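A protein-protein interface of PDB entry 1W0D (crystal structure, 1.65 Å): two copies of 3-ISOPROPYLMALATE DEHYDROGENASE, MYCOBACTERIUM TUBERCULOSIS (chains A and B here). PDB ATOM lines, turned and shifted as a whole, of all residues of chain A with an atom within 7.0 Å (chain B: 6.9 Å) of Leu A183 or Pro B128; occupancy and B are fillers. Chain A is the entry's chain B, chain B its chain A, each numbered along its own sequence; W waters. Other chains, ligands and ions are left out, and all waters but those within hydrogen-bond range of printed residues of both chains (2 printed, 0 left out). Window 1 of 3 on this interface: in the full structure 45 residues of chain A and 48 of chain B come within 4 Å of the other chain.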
ATOM      1  N   GLU A 147      34.619  27.837 -24.742  1.00  0.00           N
ATOM      2  CA  GLU A 147      33.591  27.704 -25.759  1.00  0.00           C
ATOM      3  C   GLU A 147      32.278  27.799 -25.025  1.00  0.00           C
ATOM      4  O   GLU A 147      32.116  27.219 -23.948  1.00  0.00           O
ATOM      5  CB  GLU A 147      33.694  26.326 -26.473  1.00  0.00           C
ATOM      6  CG  GLU A 147      35.047  26.075 -27.145  1.00  0.00           C
ATOM      7  CD  GLU A 147      35.210  26.822 -28.457  1.00  0.00           C
ATOM      8  OE1 GLU A 147      34.203  27.411 -28.905  1.00  0.00           O
ATOM      9  OE2 GLU A 147      36.291  26.714 -29.033  1.00  0.00           O
ATOM     10  N   SER A 149      28.092  27.566 -25.107  1.00  0.00           N
ATOM     11  CA  SER A 149      26.906  27.070 -25.754  1.00  0.00           C
ATOM     12  C   SER A 149      25.737  27.804 -25.179  1.00  0.00           C
ATOM     13  O   SER A 149      25.397  27.632 -23.995  1.00  0.00           O
ATOM     14  CB  SER A 149      26.779  25.574 -25.469  1.00  0.00           C
ATOM     15  OG  SER A 149      25.581  25.089 -26.086  1.00  0.00           O
ATOM     16  N   HIS A 178      20.631  13.944 -24.937  1.00  0.00           N
ATOM     17  CA  HIS A 178      21.399  15.047 -24.386  1.00  0.00           C
ATOM     18  C   HIS A 178      22.406  14.550 -23.408  1.00  0.00           C
ATOM     19  O   HIS A 178      22.893  13.436 -23.551  1.00  0.00           O
ATOM     20  CB  HIS A 178      20.479  16.085 -23.748  1.00  0.00           C
ATOM     21  CG  HIS A 178      21.029  17.487 -23.865  1.00  0.00           C
ATOM     22  ND1 HIS A 178      21.890  18.007 -22.930  1.00  0.00           N
ATOM     23  CD2 HIS A 178      20.847  18.470 -24.797  1.00  0.00           C
ATOM     24  CE1 HIS A 178      22.218  19.244 -23.265  1.00  0.00           C
ATOM     25  NE2 HIS A 178      21.617  19.547 -24.405  1.00  0.00           N
ATOM     26  N   LYS A 179      22.734  15.359 -22.411  1.00  0.00           N
ATOM     27  CA  LYS A 179      23.697  14.908 -21.372  1.00  0.00           C
ATOM     28  C   LYS A 179      23.347  15.674 -20.132  1.00  0.00           C
ATOM     29  O   LYS A 179      24.091  16.503 -19.612  1.00  0.00           O
ATOM     30  CB  LYS A 179      25.157  15.117 -21.758  1.00  0.00           C
ATOM     31  CG  LYS A 179      26.039  14.386 -20.773  1.00  0.00           C
ATOM     32  CD  LYS A 179      25.901  12.864 -20.917  1.00  0.00           C
ATOM     33  CE  LYS A 179      26.719  12.180 -19.819  1.00  0.00           C
ATOM     34  NZ  LYS A 179      27.420  10.963 -20.362  1.00  0.00           N
ATOM     35  N   THR A 180      22.143  15.431 -19.680  1.00  0.00           N
ATOM     36  CA  THR A 180      21.576  16.284 -18.651  1.00  0.00           C
ATOM     37  C   THR A 180      22.225  16.208 -17.286  1.00  0.00           C
ATOM     38  O   THR A 180      22.016  17.094 -16.463  1.00  0.00           O
ATOM     39  CB  THR A 180      20.141  15.930 -18.473  1.00  0.00           C
ATOM     40  OG1 THR A 180      20.029  14.545 -18.093  1.00  0.00           O
ATOM     41  CG2 THR A 180      19.421  16.034 -19.818  1.00  0.00           C
ATOM     42  N   ASN A 181      22.977  15.154 -17.026  1.00  0.00           N
ATOM     43  CA  ASN A 181      23.584  15.021 -15.714  1.00  0.00           C
ATOM     44  C   ASN A 181      24.731  15.953 -15.499  1.00  0.00           C
ATOM     45  O   ASN A 181      24.996  16.343 -14.353  1.00  0.00           O
ATOM     46  CB  ASN A 181      23.983  13.582 -15.428  1.00  0.00           C
ATOM     47  CG  ASN A 181      24.861  12.990 -16.498  1.00  0.00           C
ATOM     48  OD1 ASN A 181      24.835  13.385 -17.650  1.00  0.00           O
ATOM     49  ND2 ASN A 181      25.628  11.973 -16.117  1.00  0.00           N
ATOM     50  N   VAL A 182      25.391  16.340 -16.594  1.00  0.00           N
ATOM     51  CA  VAL A 182      26.489  17.263 -16.512  1.00  0.00           C
ATOM     52  C   VAL A 182      26.353  18.567 -17.317  1.00  0.00           C
ATOM     53  O   VAL A 182      27.039  19.550 -17.014  1.00  0.00           O
ATOM     54  CB  VAL A 182      27.738  16.550 -16.926  1.00  0.00           C
ATOM     55  CG1 VAL A 182      27.650  16.139 -18.370  1.00  0.00           C
ATOM     56  CG2 VAL A 182      28.894  17.417 -16.691  1.00  0.00           C
ATOM     57  N   LEU A 183      25.540  18.582 -18.378  1.00  0.00           N
ATOM     58  CA  LEU A 183      25.160  19.870 -18.941  1.00  0.00           C
ATOM     59  C   LEU A 183      23.842  20.185 -18.281  1.00  0.00           C
ATOM     60  O   LEU A 183      22.760  19.944 -18.852  1.00  0.00           O
ATOM     61  CB  LEU A 183      25.042  19.819 -20.463  1.00  0.00           C
ATOM     62  CG  LEU A 183      26.313  19.447 -21.207  1.00  0.00           C
ATOM     63  CD1 LEU A 183      25.978  19.375 -22.650  1.00  0.00           C
ATOM     64  CD2 LEU A 183      27.513  20.472 -20.903  1.00  0.00           C
ATOM     65  N   THR A 184      23.906  20.642 -17.027  1.00  0.00           N
ATOM     66  CA  THR A 184      22.714  20.746 -16.236  1.00  0.00           C
ATOM     67  C   THR A 184      21.754  21.817 -16.672  1.00  0.00           C
ATOM     68  O   THR A 184      20.570  21.617 -16.514  1.00  0.00           O
ATOM     69  CB  THR A 184      22.946  20.887 -14.726  1.00  0.00           C
ATOM     70  OG1 THR A 184      23.773  22.012 -14.469  1.00  0.00           O
ATOM     71  CG2 THR A 184      23.700  19.678 -14.164  1.00  0.00           C
ATOM     72  N   PHE A 185      22.276  22.920 -17.212  1.00  0.00           N
ATOM     73  CA  PHE A 185      21.440  24.088 -17.557  1.00  0.00           C
ATOM     74  C   PHE A 185      20.833  23.844 -18.913  1.00  0.00           C
ATOM     75  O   PHE A 185      19.567  23.870 -19.064  1.00  0.00           O
ATOM     76  CB  PHE A 185      22.261  25.378 -17.543  1.00  0.00           C
ATOM     77  CG  PHE A 185      22.985  25.573 -16.290  1.00  0.00           C
ATOM     78  CD1 PHE A 185      22.282  25.806 -15.103  1.00  0.00           C
ATOM     79  CD2 PHE A 185      24.325  25.367 -16.247  1.00  0.00           C
ATOM     80  CE1 PHE A 185      22.981  25.967 -13.910  1.00  0.00           C
ATOM     81  CE2 PHE A 185      25.035  25.506 -15.055  1.00  0.00           C
ATOM     82  CZ  PHE A 185      24.350  25.797 -13.891  1.00  0.00           C
ATOM     83  N   ALA A 186      21.683  23.564 -19.908  1.00  0.00           N
ATOM     84  CA  ALA A 186      21.099  23.229 -21.250  1.00  0.00           C
ATOM     85  C   ALA A 186      20.237  21.934 -21.144  1.00  0.00           C
ATOM     86  O   ALA A 186      19.158  21.833 -21.749  1.00  0.00           O
ATOM     87  CB  ALA A 186      22.206  23.031 -22.305  1.00  0.00           C
ATOM     88  N   GLY A 187      20.745  20.952 -20.395  1.00  0.00           N
ATOM     89  CA  GLY A 187      20.026  19.692 -20.205  1.00  0.00           C
ATOM     90  C   GLY A 187      18.669  19.879 -19.581  1.00  0.00           C
ATOM     91  O   GLY A 187      17.709  19.327 -20.110  1.00  0.00           O
ATOM     92  N   GLY A 188      18.581  20.646 -18.490  1.00  0.00           N
ATOM     93  CA  GLY A 188      17.334  20.851 -17.772  1.00  0.00           C
ATOM     94  C   GLY A 188      16.399  21.544 -18.734  1.00  0.00           C
ATOM     95  O   GLY A 188      15.218  21.277 -18.731  1.00  0.00           O
ATOM     96  N   LEU A 189      16.926  22.454 -19.567  1.00  0.00           N
ATOM     97  CA  LEU A 189      16.056  23.163 -20.505  1.00  0.00           C
ATOM     98  C   LEU A 189      15.500  22.209 -21.544  1.00  0.00           C
ATOM     99  O   LEU A 189      14.312  22.222 -21.789  1.00  0.00           O
ATOM    100  CB  LEU A 189      16.825  24.327 -21.181  1.00  0.00           C
ATOM    101  CG  LEU A 189      16.231  24.923 -22.459  1.00  0.00           C
ATOM    102  CD1 LEU A 189      14.913  25.580 -22.178  1.00  0.00           C
ATOM    103  CD2 LEU A 189      17.186  25.902 -23.177  1.00  0.00           C
ATOM    104  N   ASP A 231      20.400  18.364 -29.633  1.00  0.00           N
ATOM    105  CA  ASP A 231      20.813  19.729 -29.860  1.00  0.00           C
ATOM    106  C   ASP A 231      21.772  19.723 -31.016  1.00  0.00           C
ATOM    107  O   ASP A 231      22.037  18.666 -31.645  1.00  0.00           O
ATOM    108  CB  ASP A 231      21.396  20.345 -28.614  1.00  0.00           C
ATOM    109  CG  ASP A 231      22.783  19.814 -28.271  1.00  0.00           C
ATOM    110  OD1 ASP A 231      23.187  18.755 -28.800  1.00  0.00           O
ATOM    111  OD2 ASP A 231      23.561  20.387 -27.473  1.00  0.00           O
ATOM    112  N   LEU A 233      25.201  20.317 -31.264  1.00  0.00           N
ATOM    113  CA  LEU A 233      26.457  19.629 -31.110  1.00  0.00           C
ATOM    114  C   LEU A 233      26.270  18.125 -31.082  1.00  0.00           C
ATOM    115  O   LEU A 233      26.925  17.404 -31.828  1.00  0.00           O
ATOM    116  CB  LEU A 233      27.196  20.163 -29.864  1.00  0.00           C
ATOM    117  CG  LEU A 233      28.503  19.401 -29.546  1.00  0.00           C
ATOM    118  CD1 LEU A 233      29.357  20.204 -28.656  1.00  0.00           C
ATOM    119  CD2 LEU A 233      28.380  18.037 -28.880  1.00  0.00           C
ATOM    120  N   PHE A 234      25.365  17.632 -30.245  1.00  0.00           N
ATOM    121  CA  PHE A 234      25.192  16.182 -30.198  1.00  0.00           C
ATOM    122  C   PHE A 234      24.603  15.641 -31.485  1.00  0.00           C
ATOM    123  O   PHE A 234      24.958  14.560 -31.924  1.00  0.00           O
ATOM    124  CB  PHE A 234      24.293  15.781 -29.023  1.00  0.00           C
ATOM    125  CG  PHE A 234      24.890  16.084 -27.692  1.00  0.00           C
ATOM    126  CD1 PHE A 234      26.229  15.884 -27.441  1.00  0.00           C
ATOM    127  CD2 PHE A 234      24.086  16.565 -26.656  1.00  0.00           C
ATOM    128  CE1 PHE A 234      26.767  16.173 -26.173  1.00  0.00           C
ATOM    129  CE2 PHE A 234      24.632  16.830 -25.396  1.00  0.00           C
ATOM    130  CZ  PHE A 234      25.946  16.652 -25.158  1.00  0.00           C
ATOM    131  N   ARG B  81      27.641  13.404  -8.981  1.00  0.00           N
ATOM    132  CA  ARG B  81      28.352  14.677  -8.900  1.00  0.00           C
ATOM    133  C   ARG B  81      29.200  14.749  -7.612  1.00  0.00           C
ATOM    134  O   ARG B  81      30.344  15.181  -7.639  1.00  0.00           O
ATOM    135  CB  ARG B  81      27.384  15.876  -9.073  1.00  0.00           C
ATOM    136  CG  ARG B  81      26.792  16.036 -10.541  1.00  0.00           C
ATOM    137  CD  ARG B  81      26.125  17.443 -10.891  1.00  0.00           C
ATOM    138  NE  ARG B  81      26.527  18.032 -12.200  1.00  0.00           N
ATOM    139  CZ  ARG B  81      27.706  18.648 -12.470  1.00  0.00           C
ATOM    140  NH1 ARG B  81      28.656  18.751 -11.539  1.00  0.00           N
ATOM    141  NH2 ARG B  81      27.946  19.163 -13.687  1.00  0.00           N
ATOM    142  N   GLU B 126      38.524  19.074 -17.198  1.00  0.00           N
ATOM    143  CA  GLU B 126      38.021  20.369 -17.691  1.00  0.00           C
ATOM    144  C   GLU B 126      36.998  20.190 -18.784  1.00  0.00           C
ATOM    145  O   GLU B 126      36.326  19.172 -18.822  1.00  0.00           O
ATOM    146  CB  GLU B 126      39.178  21.303 -18.073  1.00  0.00           C
ATOM    147  CG  GLU B 126      40.068  20.736 -19.173  1.00  0.00           C
ATOM    148  CD  GLU B 126      41.239  21.638 -19.547  1.00  0.00           C
ATOM    149  OE1 GLU B 126      41.947  22.153 -18.649  1.00  0.00           O
ATOM    150  OE2 GLU B 126      41.445  21.782 -20.782  1.00  0.00           O
ATOM    151  N   GLY B 127      36.808  21.197 -19.624  1.00  0.00           N
ATOM    152  CA  GLY B 127      35.621  21.272 -20.486  1.00  0.00           C
ATOM    153  C   GLY B 127      34.344  21.517 -19.745  1.00  0.00           C
ATOM    154  O   GLY B 127      34.373  21.809 -18.558  1.00  0.00           O
ATOM    155  N   PRO B 128      33.205  21.272 -20.422  1.00  0.00           N
ATOM    156  CA  PRO B 128      31.854  21.667 -19.970  1.00  0.00           C
ATOM    157  C   PRO B 128      31.278  20.648 -19.026  1.00  0.00           C
ATOM    158  O   PRO B 128      30.260  20.825 -18.359  1.00  0.00           O
ATOM    159  CB  PRO B 128      31.040  21.652 -21.255  1.00  0.00           C
ATOM    160  CG  PRO B 128      31.733  20.497 -22.081  1.00  0.00           C
ATOM    161  CD  PRO B 128      33.199  20.589 -21.723  1.00  0.00           C
ATOM    162  N   TYR B 129      32.012  19.576 -18.894  1.00  0.00           N
ATOM    163  CA  TYR B 129      31.567  18.576 -17.969  1.00  0.00           C
ATOM    164  C   TYR B 129      31.782  19.067 -16.537  1.00  0.00           C
ATOM    165  O   TYR B 129      31.305  18.449 -15.571  1.00  0.00           O
ATOM    166  CB  TYR B 129      32.187  17.218 -18.326  1.00  0.00           C
ATOM    167  CG  TYR B 129      31.327  16.541 -19.402  1.00  0.00           C
ATOM    168  CD1 TYR B 129      30.198  17.202 -19.952  1.00  0.00           C
ATOM    169  CD2 TYR B 129      31.643  15.268 -19.859  1.00  0.00           C
ATOM    170  CE1 TYR B 129      29.421  16.611 -20.938  1.00  0.00           C
ATOM    171  CE2 TYR B 129      30.879  14.665 -20.815  1.00  0.00           C
ATOM    172  CZ  TYR B 129      29.758  15.325 -21.349  1.00  0.00           C
ATOM    173  OH  TYR B 129      28.972  14.718 -22.325  1.00  0.00           O
ATOM    174  N   THR B 130      32.338  20.261 -16.422  1.00  0.00           N
ATOM    175  CA  THR B 130      32.549  20.878 -15.086  1.00  0.00           C
ATOM    176  C   THR B 130      31.425  21.666 -14.428  1.00  0.00           C
ATOM    177  O   THR B 130      31.541  22.008 -13.249  1.00  0.00           O
ATOM    178  CB  THR B 130      33.811  21.785 -15.102  1.00  0.00           C
ATOM    179  OG1 THR B 130      33.499  23.012 -15.801  1.00  0.00           O
ATOM    180  CG2 THR B 130      34.932  21.124 -15.893  1.00  0.00           C
ATOM    181  N   GLY B 131      30.331  21.979 -15.114  1.00  0.00           N
ATOM    182  CA  GLY B 131      29.232  22.664 -14.417  1.00  0.00           C
ATOM    183  C   GLY B 131      29.170  24.190 -14.569  1.00  0.00           C
ATOM    184  O   GLY B 131      28.455  24.902 -13.866  1.00  0.00           O
ATOM    185  N   ASN B 132      29.924  24.670 -15.536  1.00  0.00           N
ATOM    186  CA  ASN B 132      30.132  26.094 -15.684  1.00  0.00           C
ATOM    187  C   ASN B 132      29.064  26.641 -16.605  1.00  0.00           C
ATOM    188  O   ASN B 132      28.912  26.172 -17.720  1.00  0.00           O
ATOM    189  CB  ASN B 132      31.498  26.283 -16.322  1.00  0.00           C
ATOM    190  CG  ASN B 132      32.008  27.675 -16.218  1.00  0.00           C
ATOM    191  OD1 ASN B 132      31.298  28.627 -16.473  1.00  0.00           O
ATOM    192  ND2 ASN B 132      33.305  27.799 -15.933  1.00  0.00           N
ATOM    193  N   GLU B 147      26.166  26.917 -21.317  1.00  0.00           N
ATOM    194  CA  GLU B 147      27.152  25.944 -20.877  1.00  0.00           C
ATOM    195  C   GLU B 147      28.465  26.393 -21.379  1.00  0.00           C
ATOM    196  O   GLU B 147      28.649  26.620 -22.567  1.00  0.00           O
ATOM    197  CB  GLU B 147      26.875  24.534 -21.369  1.00  0.00           C
ATOM    198  CG  GLU B 147      25.429  24.091 -21.042  1.00  0.00           C
ATOM    199  CD  GLU B 147      25.318  23.631 -19.591  1.00  0.00           C
ATOM    200  OE1 GLU B 147      26.397  23.572 -18.889  1.00  0.00           O
ATOM    201  OE2 GLU B 147      24.187  23.281 -19.178  1.00  0.00           O
ATOM    202  N   VAL B 148      29.397  26.493 -20.465  1.00  0.00           N
ATOM    203  CA  VAL B 148      30.713  26.998 -20.780  1.00  0.00           C
ATOM    204  C   VAL B 148      31.737  25.891 -20.645  1.00  0.00           C
ATOM    205  O   VAL B 148      31.808  25.218 -19.625  1.00  0.00           O
ATOM    206  CB  VAL B 148      31.077  28.148 -19.798  1.00  0.00           C
ATOM    207  CG1 VAL B 148      32.431  28.748 -20.127  1.00  0.00           C
ATOM    208  CG2 VAL B 148      29.999  29.240 -19.829  1.00  0.00           C
ATOM    209  N   SER B 149      32.543  25.729 -21.679  1.00  0.00           N
ATOM    210  CA  SER B 149      33.628  24.746 -21.635  1.00  0.00           C
ATOM    211  C   SER B 149      34.890  25.537 -21.462  1.00  0.00           C
ATOM    212  O   SER B 149      35.228  26.327 -22.315  1.00  0.00           O
ATOM    213  CB  SER B 149      33.706  23.989 -22.970  1.00  0.00           C
ATOM    214  OG  SER B 149      34.879  23.192 -23.139  1.00  0.00           O
ATOM    215  N   VAL B 150      35.618  25.238 -20.399  1.00  0.00           N
ATOM    216  CA  VAL B 150      36.896  25.883 -20.141  1.00  0.00           C
ATOM    217  C   VAL B 150      37.995  24.883 -20.441  1.00  0.00           C
ATOM    218  O   VAL B 150      37.928  23.771 -20.016  1.00  0.00           O
ATOM    219  CB  VAL B 150      36.987  26.352 -18.727  1.00  0.00           C
ATOM    220  CG1 VAL B 150      38.323  27.045 -18.447  1.00  0.00           C
ATOM    221  CG2 VAL B 150      35.804  27.324 -18.458  1.00  0.00           C
ATOM    222  N   ASN B 151      38.935  25.274 -21.296  1.00  0.00           N
ATOM    223  CA  ASN B 151      39.990  24.407 -21.756  1.00  0.00           C
ATOM    224  C   ASN B 151      41.279  25.121 -21.496  1.00  0.00           C
ATOM    225  O   ASN B 151      41.359  26.336 -21.624  1.00  0.00           O
ATOM    226  CB  ASN B 151      39.834  24.218 -23.260  1.00  0.00           C
ATOM    227  CG  ASN B 151      38.472  23.645 -23.581  1.00  0.00           C
ATOM    228  OD1 ASN B 151      38.333  22.425 -23.601  1.00  0.00           O
ATOM    229  ND2 ASN B 151      37.429  24.504 -23.701  1.00  0.00           N
ATOM    230  N   ASP B 231      38.955  15.416 -25.771  1.00  0.00           N
ATOM    231  CA  ASP B 231      38.609  16.151 -24.600  1.00  0.00           C
ATOM    232  C   ASP B 231      37.553  15.399 -23.779  1.00  0.00           C
ATOM    233  O   ASP B 231      37.206  14.253 -24.045  1.00  0.00           O
ATOM    234  CB  ASP B 231      38.154  17.562 -24.945  1.00  0.00           C
ATOM    235  CG  ASP B 231      36.737  17.623 -25.497  1.00  0.00           C
ATOM    236  OD1 ASP B 231      36.154  16.583 -25.899  1.00  0.00           O
ATOM    237  OD2 ASP B 231      36.116  18.709 -25.574  1.00  0.00           O
ATOM    238  N   ASN B 232      37.092  16.081 -22.759  1.00  0.00           N
ATOM    239  CA  ASN B 232      36.230  15.435 -21.783  1.00  0.00           C
ATOM    240  C   ASN B 232      34.885  15.088 -22.428  1.00  0.00           C
ATOM    241  O   ASN B 232      34.384  13.970 -22.271  1.00  0.00           O
ATOM    242  CB  ASN B 232      36.141  16.411 -20.644  1.00  0.00           C
ATOM    243  CG  ASN B 232      35.793  15.794 -19.342  1.00  0.00           C
ATOM    244  OD1 ASN B 232      35.384  14.660 -19.267  1.00  0.00           O
ATOM    245  ND2 ASN B 232      35.992  16.558 -18.286  1.00  0.00           N
ATOM    246  N   LEU B 233      34.269  16.021 -23.154  1.00  0.00           N
ATOM    247  CA  LEU B 233      32.953  15.761 -23.675  1.00  0.00           C
ATOM    248  C   LEU B 233      32.978  14.757 -24.803  1.00  0.00           C
ATOM    249  O   LEU B 233      32.237  13.777 -24.767  1.00  0.00           O
ATOM    250  CB  LEU B 233      32.290  17.065 -24.127  1.00  0.00           C
ATOM    251  CG  LEU B 233      30.881  16.910 -24.706  1.00  0.00           C
ATOM    252  CD1 LEU B 233      30.283  18.281 -24.786  1.00  0.00           C
ATOM    253  CD2 LEU B 233      30.824  16.274 -26.067  1.00  0.00           C
HETATM  254  O   HOH W   1      30.222  24.722 -24.229  1.00  0.00           O
HETATM  255  O   HOH W   2      26.250  22.417 -16.501  1.00  0.00           O
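O of Glu A147 touches O of Glu B147, 3.8 Å away. O of Glu A147 touches CA of Val B148 (3.5 Å). CG of Lys A179 touches OH of Tyr B129, at 3.3 Å. O of Val A182 touches O of Pro B128, 3.7 Å away. Val A182 touches Tyr B129. CD2 of Leu A183 touches CB of Pro B128, 3.7 Å away. Glu B147 touches Leu A183 (OE2 to C, 3.2 Å). Thr A184 touches Arg B81. Phe A185 touches Gly B131 (CE2 to O, 3.7 Å).
Hydrophobic or aromatic side chains of chain A that line the printed part of chain B: Val A182, Leu A183, Phe A185 and Ala A186. Printed residues of chain B that touch a printed residue of chain A: Arg B81, Pro B128, Tyr B129, Gly B131, Glu B147, Val B148 and Ser B149. Hydrophobic or aromatic side chains of chain B within 4 Å of the printed part of chain A: Pro B128 and Tyr B129. Along chain B the printed residues that touch a printed residue of chain A span positions 81 to 149. Among the printed residues, 16 pairs touch across the chains. Among the printed residues, no Asp or Glu carboxylate lies within 4 Å of a Lys or Arg side-chain nitrogen of the other chain.
Leu A183 touches just these residues of chain B: Pro B128 and Glu B147. Pro B128 touches just these residues of chain A: Val A182 and Leu A183. Of the printed residues of chain A, Gly B131 touches Phe A185 (3.7 Å). Of the printed residues of chain B, Lys A179 touches Tyr B129 (3.3 Å). Printed residues of chain B within 4 Å of Ala A186: Glu B147. Printed residues of chain A within 4 Å of Tyr B129: Lys A179 and Val A182. Of the printed residues of chain B, Thr A184 touches Arg B81 and Glu B147. Leu B233 touches none of the printed residues of chain A. The nearest residue of chain B that does not touch Leu A183 is Tyr B129 (4.2 Å).
Glu A147 touches its own counterpart, Glu B147. Glu A147 touches Ser B149, and with the chains exchanged Ser A149 touches Glu B147. Positions printed for both chains: 147, 149, 231 and 233. Of the 16 pairs that touch across the chains among the printed residues, 3 have their exchanged pair printed and touching as well.
The backbone carbonyl oxygen (O) of Asn B132 lies within hydrogen-bond range of the backbone NH (N) of Val B148 (2.8 Å). The side-chain amide nitrogen (ND2) of Asn B151 lies within hydrogen-bond range of the side-chain hydroxyl (OG) of Ser B149 (2.9 Å).
N of Ser B149 is in hydrogen-bond range of O of Glu A147 (2.7 Å). OE2 of Glu B147 sits at hydrogen-bond distance from N of Ala A186 (2.6 Å). The side-chain carboxylate (OE2) of Glu B147 lies within hydrogen-bond range of the backbone NH (N) of Phe A185. OE2 of Glu B147 lies within hydrogen-bond range of N of Thr A184, at 3.4 Å. The guanidinium group of Arg B81 is in hydrogen-bond range of the backbone carbonyl oxygen of Val A182. The guanidinium group (NE) of Arg B81 is in hydrogen-bond range of the backbone carbonyl oxygen (O) of Asn A181. N of Ser A149 is in hydrogen-bond range of O of Glu B147, 2.8 Å away.
Water W2 lies within hydrogen-bond range of the side-chain carboxylate of Glu B147 (2.7 Å), the backbone NH of Thr A184 (3.0 Å) and the backbone carbonyl oxygen of Val A182 (3.0 Å). Water W1 lies within hydrogen-bond range of the backbone carbonyl oxygen (O) of Glu B147 (3.0 Å) and the backbone carbonyl oxygen (O) of Glu A147 (3.1 Å).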
